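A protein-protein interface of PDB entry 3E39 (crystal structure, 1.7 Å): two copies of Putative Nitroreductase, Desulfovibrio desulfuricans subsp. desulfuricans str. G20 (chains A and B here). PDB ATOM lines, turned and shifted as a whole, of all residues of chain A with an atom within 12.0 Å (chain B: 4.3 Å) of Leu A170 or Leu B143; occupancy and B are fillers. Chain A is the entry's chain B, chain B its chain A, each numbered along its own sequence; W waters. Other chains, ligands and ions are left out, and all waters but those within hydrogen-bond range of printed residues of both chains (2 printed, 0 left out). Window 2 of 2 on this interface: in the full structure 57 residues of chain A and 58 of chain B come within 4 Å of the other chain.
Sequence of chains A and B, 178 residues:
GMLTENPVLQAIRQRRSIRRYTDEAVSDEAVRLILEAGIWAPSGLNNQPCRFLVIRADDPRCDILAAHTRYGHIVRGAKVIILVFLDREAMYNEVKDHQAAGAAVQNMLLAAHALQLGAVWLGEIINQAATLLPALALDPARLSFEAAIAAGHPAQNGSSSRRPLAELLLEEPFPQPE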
ATOM      1  N   VAL A  95       7.926  -4.317 -11.893  1.00  0.00           N
ATOM      2  CA  VAL A  95       6.845  -3.362 -12.219  1.00  0.00           C
ATOM      3  C   VAL A  95       5.798  -3.256 -11.101  1.00  0.00           C
ATOM      4  O   VAL A  95       5.473  -2.154 -10.655  1.00  0.00           O
ATOM      5  CB  VAL A  95       6.153  -3.708 -13.520  1.00  0.00           C
ATOM      6  CG1 VAL A  95       4.832  -2.917 -13.667  1.00  0.00           C
ATOM      7  CG2 VAL A  95       7.109  -3.459 -14.734  1.00  0.00           C
ATOM      8  N   GLN A  99       4.749  -0.187  -8.518  1.00  0.00           N
ATOM      9  CA  GLN A  99       3.359   0.302  -8.411  1.00  0.00           C
ATOM     10  C   GLN A  99       2.975   0.352  -6.925  1.00  0.00           C
ATOM     11  O   GLN A  99       2.340   1.296  -6.444  1.00  0.00           O
ATOM     12  CB  GLN A  99       2.400  -0.624  -9.136  1.00  0.00           C
ATOM     13  CG  GLN A  99       2.549  -0.634 -10.644  1.00  0.00           C
ATOM     14  CD  GLN A  99       1.713  -1.708 -11.284  1.00  0.00           C
ATOM     15  OE1 GLN A  99       1.303  -2.678 -10.623  1.00  0.00           O
ATOM     16  NE2 GLN A  99       1.400  -1.526 -12.579  1.00  0.00           N
ATOM     17  N   ARG A 163      -6.214  17.125 -17.359  1.00  0.00           N
ATOM     18  CA  ARG A 163      -7.005  17.073 -18.599  1.00  0.00           C
ATOM     19  C   ARG A 163      -8.337  16.393 -18.241  1.00  0.00           C
ATOM     20  O   ARG A 163      -8.426  15.682 -17.210  1.00  0.00           O
ATOM     21  CB  ARG A 163      -6.242  16.320 -19.687  1.00  0.00           C
ATOM     22  CG  ARG A 163      -4.900  16.926 -19.957  1.00  0.00           C
ATOM     23  CD  ARG A 163      -4.249  16.489 -21.238  1.00  0.00           C
ATOM     24  NE  ARG A 163      -3.756  15.117 -21.162  1.00  0.00           N
ATOM     25  CZ  ARG A 163      -4.169  14.096 -21.914  1.00  0.00           C
ATOM     26  NH1 ARG A 163      -5.090  14.251 -22.858  1.00  0.00           N
ATOM     27  NH2 ARG A 163      -3.618  12.901 -21.731  1.00  0.00           N
ATOM     28  N   PRO A 164      -9.401  16.611 -19.059  1.00  0.00           N
ATOM     29  CA  PRO A 164     -10.690  16.050 -18.719  1.00  0.00           C
ATOM     30  C   PRO A 164     -10.666  14.540 -18.770  1.00  0.00           C
ATOM     31  O   PRO A 164      -9.966  13.970 -19.594  1.00  0.00           O
ATOM     32  CB  PRO A 164     -11.638  16.602 -19.785  1.00  0.00           C
ATOM     33  CG  PRO A 164     -10.891  17.798 -20.394  1.00  0.00           C
ATOM     34  CD  PRO A 164      -9.457  17.389 -20.326  1.00  0.00           C
ATOM     35  N   LEU A 165     -11.430  13.920 -17.878  1.00  0.00           N
ATOM     36  CA  LEU A 165     -11.539  12.459 -17.835  1.00  0.00           C
ATOM     37  C   LEU A 165     -11.770  11.830 -19.215  1.00  0.00           C
ATOM     38  O   LEU A 165     -11.157  10.804 -19.560  1.00  0.00           O
ATOM     39  CB  LEU A 165     -12.673  12.052 -16.878  1.00  0.00           C
ATOM     40  CG  LEU A 165     -12.974  10.552 -16.790  1.00  0.00           C
ATOM     41  CD1 LEU A 165     -11.696   9.729 -16.482  1.00  0.00           C
ATOM     42  CD2 LEU A 165     -14.027  10.307 -15.734  1.00  0.00           C
ATOM     43  N   ALA A 166     -12.644  12.431 -20.016  1.00  0.00           N
ATOM     44  CA  ALA A 166     -12.987  11.865 -21.314  1.00  0.00           C
ATOM     45  C   ALA A 166     -11.797  11.683 -22.225  1.00  0.00           C
ATOM     46  O   ALA A 166     -11.777  10.759 -23.054  1.00  0.00           O
ATOM     47  CB  ALA A 166     -14.092  12.697 -22.007  1.00  0.00           C
ATOM     48  N   GLU A 167     -10.792  12.551 -22.087  1.00  0.00           N
ATOM     49  CA  GLU A 167      -9.561  12.396 -22.869  1.00  0.00           C
ATOM     50  C   GLU A 167      -8.685  11.229 -22.435  1.00  0.00           C
ATOM     51  O   GLU A 167      -7.920  10.714 -23.239  1.00  0.00           O
ATOM     52  CB  GLU A 167      -8.714  13.663 -22.798  1.00  0.00           C
ATOM     53  CG  GLU A 167      -9.346  14.822 -23.534  1.00  0.00           C
ATOM     54  CD  GLU A 167      -8.468  16.048 -23.580  1.00  0.00           C
ATOM     55  OE1 GLU A 167      -7.264  16.025 -23.170  1.00  0.00           O
ATOM     56  OE2 GLU A 167      -8.997  17.079 -23.985  1.00  0.00           O
ATOM     57  N   LEU A 168      -8.788  10.819 -21.172  1.00  0.00           N
ATOM     58  CA  LEU A 168      -7.939   9.732 -20.657  1.00  0.00           C
ATOM     59  C   LEU A 168      -8.580   8.352 -20.790  1.00  0.00           C
ATOM     60  O   LEU A 168      -7.973   7.340 -20.436  1.00  0.00           O
ATOM     61  CB  LEU A 168      -7.593   9.987 -19.202  1.00  0.00           C
ATOM     62  CG  LEU A 168      -7.100  11.391 -18.859  1.00  0.00           C
ATOM     63  CD1 LEU A 168      -6.640  11.434 -17.416  1.00  0.00           C
ATOM     64  CD2 LEU A 168      -6.004  11.792 -19.766  1.00  0.00           C
ATOM     65  N   LEU A 169      -9.843   8.328 -21.182  1.00  0.00           N
ATOM     66  CA  LEU A 169     -10.567   7.103 -21.413  1.00  0.00           C
ATOM     67  C   LEU A 169     -10.335   6.609 -22.809  1.00  0.00           C
ATOM     68  O   LEU A 169     -10.456   7.363 -23.769  1.00  0.00           O
ATOM     69  CB  LEU A 169     -12.048   7.323 -21.197  1.00  0.00           C
ATOM     70  CG  LEU A 169     -12.524   7.358 -19.748  1.00  0.00           C
ATOM     71  CD1 LEU A 169     -13.839   8.095 -19.720  1.00  0.00           C
ATOM     72  CD2 LEU A 169     -12.619   5.895 -19.170  1.00  0.00           C
ATOM     73  N   LEU A 170     -10.030   5.326 -22.923  1.00  0.00           N
ATOM     74  CA  LEU A 170      -9.798   4.728 -24.212  1.00  0.00           C
ATOM     75  C   LEU A 170     -11.080   4.540 -25.023  1.00  0.00           C
ATOM     76  O   LEU A 170     -11.034   4.337 -26.243  1.00  0.00           O
ATOM     77  CB  LEU A 170      -9.071   3.405 -24.048  1.00  0.00           C
ATOM     78  CG  LEU A 170      -7.656   3.497 -23.426  1.00  0.00           C
ATOM     79  CD1 LEU A 170      -7.040   2.120 -23.296  1.00  0.00           C
ATOM     80  CD2 LEU A 170      -6.752   4.428 -24.229  1.00  0.00           C
ATOM     81  N   GLU A 171     -12.214   4.569 -24.339  1.00  0.00           N
ATOM     82  CA  GLU A 171     -13.518   4.438 -24.958  1.00  0.00           C
ATOM     83  C   GLU A 171     -14.443   5.191 -24.028  1.00  0.00           C
ATOM     84  O   GLU A 171     -14.235   5.194 -22.804  1.00  0.00           O
ATOM     85  CB  GLU A 171     -13.876   2.960 -25.037  1.00  0.00           C
ATOM     86  CG  GLU A 171     -15.286   2.645 -25.377  1.00  0.00           C
ATOM     87  CD  GLU A 171     -15.480   1.169 -25.398  1.00  0.00           C
ATOM     88  OE1 GLU A 171     -14.912   0.521 -26.294  1.00  0.00           O
ATOM     89  OE2 GLU A 171     -16.164   0.658 -24.489  1.00  0.00           O
ATOM     90  N   GLU A 172     -15.442   5.861 -24.581  1.00  0.00           N
ATOM     91  CA  GLU A 172     -16.354   6.631 -23.738  1.00  0.00           C
ATOM     92  C   GLU A 172     -17.416   5.676 -23.169  1.00  0.00           C
ATOM     93  O   GLU A 172     -18.174   5.090 -23.931  1.00  0.00           O
ATOM     94  CB  GLU A 172     -16.949   7.803 -24.529  1.00  0.00           C
ATOM     95  CG  GLU A 172     -15.888   8.732 -25.210  1.00  0.00           C
ATOM     96  CD  GLU A 172     -14.777   9.300 -24.276  1.00  0.00           C
ATOM     97  OE1 GLU A 172     -14.956   9.347 -23.053  1.00  0.00           O
ATOM     98  OE2 GLU A 172     -13.716   9.729 -24.792  1.00  0.00           O
ATOM     99  N   PRO A 173     -17.464   5.497 -21.831  1.00  0.00           N
ATOM    100  CA  PRO A 173     -18.352   4.508 -21.212  1.00  0.00           C
ATOM    101  C   PRO A 173     -19.757   4.965 -20.788  1.00  0.00           C
ATOM    102  O   PRO A 173     -20.579   4.125 -20.423  1.00  0.00           O
ATOM    103  CB  PRO A 173     -17.564   4.120 -19.971  1.00  0.00           C
ATOM    104  CG  PRO A 173     -17.022   5.434 -19.504  1.00  0.00           C
ATOM    105  CD  PRO A 173     -16.663   6.183 -20.805  1.00  0.00           C
ATOM    106  N   PHE A 174     -20.038   6.265 -20.840  1.00  0.00           N
ATOM    107  CA  PHE A 174     -21.329   6.779 -20.385  1.00  0.00           C
ATOM    108  C   PHE A 174     -22.252   7.130 -21.561  1.00  0.00           C
ATOM    109  O   PHE A 174     -21.784   7.317 -22.684  1.00  0.00           O
ATOM    110  CB  PHE A 174     -21.096   7.981 -19.464  1.00  0.00           C
ATOM    111  CG  PHE A 174     -20.118   7.705 -18.352  1.00  0.00           C
ATOM    112  CD1 PHE A 174     -20.352   6.659 -17.456  1.00  0.00           C
ATOM    113  CD2 PHE A 174     -18.981   8.493 -18.179  1.00  0.00           C
ATOM    114  CE1 PHE A 174     -19.473   6.402 -16.415  1.00  0.00           C
ATOM    115  CE2 PHE A 174     -18.084   8.227 -17.130  1.00  0.00           C
ATOM    116  CZ  PHE A 174     -18.334   7.194 -16.253  1.00  0.00           C
ATOM    117  N   ARG B  51      -4.251   5.906 -18.630  1.00  0.00           N
ATOM    118  CA  ARG B  51      -5.401   5.773 -19.525  1.00  0.00           C
ATOM    119  C   ARG B  51      -6.287   4.664 -18.930  1.00  0.00           C
ATOM    120  O   ARG B  51      -5.784   3.748 -18.272  1.00  0.00           O
ATOM    121  CB  ARG B  51      -4.949   5.415 -20.930  1.00  0.00           C
ATOM    122  CG  ARG B  51      -4.068   6.451 -21.599  1.00  0.00           C
ATOM    123  CD  ARG B  51      -4.791   7.785 -21.873  1.00  0.00           C
ATOM    124  NE  ARG B  51      -3.833   8.692 -22.533  1.00  0.00           N
ATOM    125  CZ  ARG B  51      -2.975   9.496 -21.905  1.00  0.00           C
ATOM    126  NH1 ARG B  51      -2.995   9.624 -20.594  1.00  0.00           N
ATOM    127  NH2 ARG B  51      -2.118  10.244 -22.620  1.00  0.00           N
ATOM    128  N   PHE B  52      -7.583   4.739 -19.200  1.00  0.00           N
ATOM    129  CA  PHE B  52      -8.554   3.854 -18.553  1.00  0.00           C
ATOM    130  C   PHE B  52      -9.547   3.291 -19.535  1.00  0.00           C
ATOM    131  O   PHE B  52      -9.917   3.952 -20.523  1.00  0.00           O
ATOM    132  CB  PHE B  52      -9.303   4.634 -17.471  1.00  0.00           C
ATOM    133  CG  PHE B  52      -8.380   5.401 -16.555  1.00  0.00           C
ATOM    134  CD1 PHE B  52      -7.841   4.811 -15.436  1.00  0.00           C
ATOM    135  CD2 PHE B  52      -7.972   6.699 -16.877  1.00  0.00           C
ATOM    136  CE1 PHE B  52      -6.982   5.514 -14.605  1.00  0.00           C
ATOM    137  CE2 PHE B  52      -7.088   7.393 -16.040  1.00  0.00           C
ATOM    138  CZ  PHE B  52      -6.615   6.793 -14.901  1.00  0.00           C
ATOM    139  N   PHE B  85      -3.911   1.674 -17.804  1.00  0.00           N
ATOM    140  CA  PHE B  85      -2.773   1.598 -18.700  1.00  0.00           C
ATOM    141  C   PHE B  85      -1.921   2.860 -18.586  1.00  0.00           C
ATOM    142  O   PHE B  85      -2.338   3.893 -18.041  1.00  0.00           O
ATOM    143  CB  PHE B  85      -3.206   1.553 -20.182  1.00  0.00           C
ATOM    144  CG  PHE B  85      -4.220   0.504 -20.497  1.00  0.00           C
ATOM    145  CD1 PHE B  85      -5.567   0.754 -20.276  1.00  0.00           C
ATOM    146  CD2 PHE B  85      -3.841  -0.719 -21.036  1.00  0.00           C
ATOM    147  CE1 PHE B  85      -6.509  -0.204 -20.541  1.00  0.00           C
ATOM    148  CE2 PHE B  85      -4.794  -1.680 -21.310  1.00  0.00           C
ATOM    149  CZ  PHE B  85      -6.118  -1.426 -21.067  1.00  0.00           C
ATOM    150  N   LEU B  86      -0.687   2.749 -19.046  1.00  0.00           N
ATOM    151  CA  LEU B  86       0.122   3.925 -19.295  1.00  0.00           C
ATOM    152  C   LEU B  86       0.192   4.080 -20.811  1.00  0.00           C
ATOM    153  O   LEU B  86       0.361   3.104 -21.561  1.00  0.00           O
ATOM    154  CB  LEU B  86       1.546   3.822 -18.758  1.00  0.00           C
ATOM    155  CG  LEU B  86       1.709   3.779 -17.248  1.00  0.00           C
ATOM    156  CD1 LEU B  86       3.083   3.366 -16.854  1.00  0.00           C
ATOM    157  CD2 LEU B  86       1.359   5.145 -16.671  1.00  0.00           C
ATOM    158  N   ASP B  87       0.032   5.316 -21.249  1.00  0.00           N
ATOM    159  CA  ASP B  87       0.221   5.682 -22.652  1.00  0.00           C
ATOM    160  C   ASP B  87       1.728   5.784 -22.853  1.00  0.00           C
ATOM    161  O   ASP B  87       2.403   6.640 -22.275  1.00  0.00           O
ATOM    162  CB  ASP B  87      -0.473   7.003 -22.933  1.00  0.00           C
ATOM    163  CG  ASP B  87      -0.284   7.487 -24.373  1.00  0.00           C
ATOM    164  OD1 ASP B  87       0.702   7.133 -25.032  1.00  0.00           O
ATOM    165  OD2 ASP B  87      -1.105   8.282 -24.824  1.00  0.00           O
ATOM    166  N   ARG B  88       2.274   4.910 -23.675  1.00  0.00           N
ATOM    167  CA  ARG B  88       3.724   4.890 -23.910  1.00  0.00           C
ATOM    168  C   ARG B  88       4.283   6.194 -24.460  1.00  0.00           C
ATOM    169  O   ARG B  88       5.445   6.504 -24.202  1.00  0.00           O
ATOM    170  CB  ARG B  88       4.123   3.716 -24.808  1.00  0.00           C
ATOM    171  CG  ARG B  88       3.845   2.368 -24.149  1.00  0.00           C
ATOM    172  CD  ARG B  88       4.317   1.178 -24.988  1.00  0.00           C
ATOM    173  NE  ARG B  88       3.937  -0.099 -24.392  1.00  0.00           N
ATOM    174  CZ  ARG B  88       4.616  -0.734 -23.435  1.00  0.00           C
ATOM    175  NH1 ARG B  88       5.723  -0.218 -22.918  1.00  0.00           N
ATOM    176  NH2 ARG B  88       4.155  -1.870 -22.957  1.00  0.00           N
ATOM    177  N   LEU B 133      -4.191  -7.718 -24.834  1.00  0.00           N
ATOM    178  CA  LEU B 133      -4.458  -6.411 -25.436  1.00  0.00           C
ATOM    179  C   LEU B 133      -4.960  -6.506 -26.877  1.00  0.00           C
ATOM    180  O   LEU B 133      -5.999  -5.919 -27.202  1.00  0.00           O
ATOM    181  CB  LEU B 133      -3.259  -5.461 -25.271  1.00  0.00           C
ATOM    182  CG  LEU B 133      -3.349  -4.553 -24.025  1.00  0.00           C
ATOM    183  CD1 LEU B 133      -3.502  -5.367 -22.705  1.00  0.00           C
ATOM    184  CD2 LEU B 133      -2.166  -3.556 -23.938  1.00  0.00           C
ATOM    185  N   LEU B 138      -6.639  -3.522 -28.620  1.00  0.00           N
ATOM    186  CA  LEU B 138      -5.688  -2.509 -28.119  1.00  0.00           C
ATOM    187  C   LEU B 138      -4.265  -2.831 -28.607  1.00  0.00           C
ATOM    188  O   LEU B 138      -3.910  -3.981 -28.836  1.00  0.00           O
ATOM    189  CB  LEU B 138      -5.743  -2.413 -26.591  1.00  0.00           C
ATOM    190  CG  LEU B 138      -7.105  -2.082 -25.973  1.00  0.00           C
ATOM    191  CD1 LEU B 138      -7.094  -2.162 -24.425  1.00  0.00           C
ATOM    192  CD2 LEU B 138      -7.564  -0.707 -26.452  1.00  0.00           C
ATOM    193  N   ASP B 139      -3.458  -1.794 -28.739  1.00  0.00           N
ATOM    194  CA  ASP B 139      -2.122  -1.900 -29.291  1.00  0.00           C
ATOM    195  C   ASP B 139      -1.076  -1.887 -28.167  1.00  0.00           C
ATOM    196  O   ASP B 139      -0.914  -0.864 -27.505  1.00  0.00           O
ATOM    197  CB  ASP B 139      -1.931  -0.701 -30.229  1.00  0.00           C
ATOM    198  CG  ASP B 139      -0.622  -0.727 -30.989  1.00  0.00           C
ATOM    199  OD1 ASP B 139       0.117  -1.720 -30.908  1.00  0.00           O
ATOM    200  OD2 ASP B 139      -0.377   0.286 -31.686  1.00  0.00           O
ATOM    201  N   PRO B 140      -0.395  -3.022 -27.943  1.00  0.00           N
ATOM    202  CA  PRO B 140       0.640  -3.031 -26.914  1.00  0.00           C
ATOM    203  C   PRO B 140       1.818  -2.104 -27.225  1.00  0.00           C
ATOM    204  O   PRO B 140       2.612  -1.818 -26.330  1.00  0.00           O
ATOM    205  CB  PRO B 140       1.093  -4.501 -26.858  1.00  0.00           C
ATOM    206  CG  PRO B 140       0.093  -5.285 -27.647  1.00  0.00           C
ATOM    207  CD  PRO B 140      -0.526  -4.339 -28.605  1.00  0.00           C
ATOM    208  N   ALA B 141       1.948  -1.643 -28.471  1.00  0.00           N
ATOM    209  CA  ALA B 141       3.007  -0.703 -28.824  1.00  0.00           C
ATOM    210  C   ALA B 141       2.620   0.703 -28.363  1.00  0.00           C
ATOM    211  O   ALA B 141       3.469   1.598 -28.257  1.00  0.00           O
ATOM    212  CB  ALA B 141       3.265  -0.726 -30.344  1.00  0.00           C
ATOM    213  N   ARG B 142       1.341   0.907 -28.062  1.00  0.00           N
ATOM    214  CA  ARG B 142       0.869   2.209 -27.610  1.00  0.00           C
ATOM    215  C   ARG B 142       0.615   2.257 -26.115  1.00  0.00           C
ATOM    216  O   ARG B 142       0.745   3.317 -25.507  1.00  0.00           O
ATOM    217  CB  ARG B 142      -0.432   2.591 -28.280  1.00  0.00           C
ATOM    218  CG  ARG B 142      -0.925   3.996 -27.902  1.00  0.00           C
ATOM    219  CD  ARG B 142       0.196   5.086 -28.081  1.00  0.00           C
ATOM    220  NE  ARG B 142      -0.223   6.404 -27.618  1.00  0.00           N
ATOM    221  CZ  ARG B 142      -1.095   7.176 -28.259  1.00  0.00           C
ATOM    222  NH1 ARG B 142      -1.662   6.781 -29.403  1.00  0.00           N
ATOM    223  NH2 ARG B 142      -1.419   8.352 -27.746  1.00  0.00           N
ATOM    224  N   LEU B 143       0.243   1.109 -25.547  1.00  0.00           N
ATOM    225  CA  LEU B 143      -0.174   1.057 -24.152  1.00  0.00           C
ATOM    226  C   LEU B 143       0.547  -0.003 -23.339  1.00  0.00           C
ATOM    227  O   LEU B 143       0.809  -1.097 -23.851  1.00  0.00           O
ATOM    228  CB  LEU B 143      -1.681   0.741 -24.151  1.00  0.00           C
ATOM    229  CG  LEU B 143      -2.650   1.736 -24.835  1.00  0.00           C
ATOM    230  CD1 LEU B 143      -4.023   1.058 -25.034  1.00  0.00           C
ATOM    231  CD2 LEU B 143      -2.740   3.043 -24.057  1.00  0.00           C
ATOM    232  N   SER B 144       0.903   0.343 -22.095  1.00  0.00           N
ATOM    233  CA  SER B 144       1.448  -0.581 -21.111  1.00  0.00           C
ATOM    234  C   SER B 144       0.289  -0.891 -20.157  1.00  0.00           C
ATOM    235  O   SER B 144      -0.286   0.028 -19.589  1.00  0.00           O
ATOM    236  CB  SER B 144       2.609   0.044 -20.337  1.00  0.00           C
ATOM    237  OG  SER B 144       2.912  -0.744 -19.222  1.00  0.00           O
ATOM    238  N   PHE B 145      -0.060  -2.169 -20.029  1.00  0.00           N
ATOM    239  CA  PHE B 145      -1.157  -2.611 -19.213  1.00  0.00           C
ATOM    240  C   PHE B 145      -0.655  -2.681 -17.783  1.00  0.00           C
ATOM    241  O   PHE B 145       0.229  -3.482 -17.484  1.00  0.00           O
ATOM    242  CB  PHE B 145      -1.676  -3.955 -19.752  1.00  0.00           C
ATOM    243  CG  PHE B 145      -2.845  -4.540 -19.003  1.00  0.00           C
ATOM    244  CD1 PHE B 145      -3.828  -3.743 -18.412  1.00  0.00           C
ATOM    245  CD2 PHE B 145      -3.011  -5.929 -18.961  1.00  0.00           C
ATOM    246  CE1 PHE B 145      -4.902  -4.313 -17.735  1.00  0.00           C
ATOM    247  CE2 PHE B 145      -4.105  -6.495 -18.309  1.00  0.00           C
ATOM    248  CZ  PHE B 145      -5.056  -5.685 -17.700  1.00  0.00           C
HETATM  249  O   HOH W   1      -0.738  12.596 -21.477  1.00  0.00           O
HETATM  250  O   HOH W   2      -5.115  11.339 -24.038  1.00  0.00           O
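No position is printed for both chains. Of the 8 pairs that touch across the chains among the printed residues, none has its exchanged pair printed and touching as well.
Of the printed residues of chain B, Arg A163 touches Arg B51 (3.2 Å). Leu A165 touches none of the printed residues of chain B. Leu A170 touches just these residues of chain B: Arg B51 (3.9 Å), Phe B52 (2.8 Å), Phe B85 (3.6 Å) and Leu B143 (3.6 Å). Of the printed residues of chain A, Phe B52 touches Leu A168 (2.9 Å), Leu A169 (3.3 Å) and Leu A170 (2.8 Å). Phe B85 touches one residue of chain A. No residue of chain A comes within 4 Å of Asp B87. No residue of chain A comes within 4 Å of Arg B88. No residue of chain A comes within 4 Å of Leu B138. No residue of chain A comes within 4 Å of Asp B139. No residue of chain A comes within 4 Å of Arg B142. Ser B144 touches none of the printed residues of chain A.
The backbone NH of Phe B52 sits at hydrogen-bond distance from the backbone carbonyl oxygen of Leu A168 (2.9 Å). The backbone NH (N) of Leu A170 sits at hydrogen-bond distance from the backbone carbonyl oxygen (O) of Phe B52. The guanidinium group (NH2) of Arg A163 lies close to the guanidinium group (NH2) of Arg B51, 3.2 Å away.
Among the printed residues, pairs that only touch across the chains: Leu A168 with Arg B51, Leu A169 with Phe B52, Leu A170 with Arg B51, Leu A170 with Phe B85 and Leu A170 with Leu B143.
Water W1 lies within hydrogen-bond range of the guanidinium group of Arg A163 and the guanidinium group of Arg B51. Water W2 lies within hydrogen-bond range of the backbone carbonyl oxygen of Glu A167, the guanidinium group of Arg A163 and the guanidinium group of Arg B51.
Hydrophobic or aromatic side chains of chain B within 4 Å of the printed part of chain A: Phe B52, Phe B85 and Leu B143. Of the 14 printed residues of chain A, 4 touch a printed residue of chain B. Hydrophobic or aromatic side chains of chain A within 4 Å of the printed part of chain B: Leu A168, Leu A169 and Leu A170. Among the printed residues, no Asp or Glu carboxylate lies within 4 Å of a Lys or Arg side-chain nitrogen of the other chain.
O of Arg B51 sits at hydrogen-bond distance from N of Phe B85, at 2.8 Å. NH2 of Arg B51 lies within salt-bridge range of OD2 of Asp B87 (3.1 Å). The guanidinium group (NE) of Arg B88 sits at hydrogen-bond distance from the backbone carbonyl oxygen (O) of Leu B143 (3.3 Å). The guanidinium group (NH1) of Arg A163 is in salt-bridge range of the side-chain carboxylate (OE1) of Glu A167.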
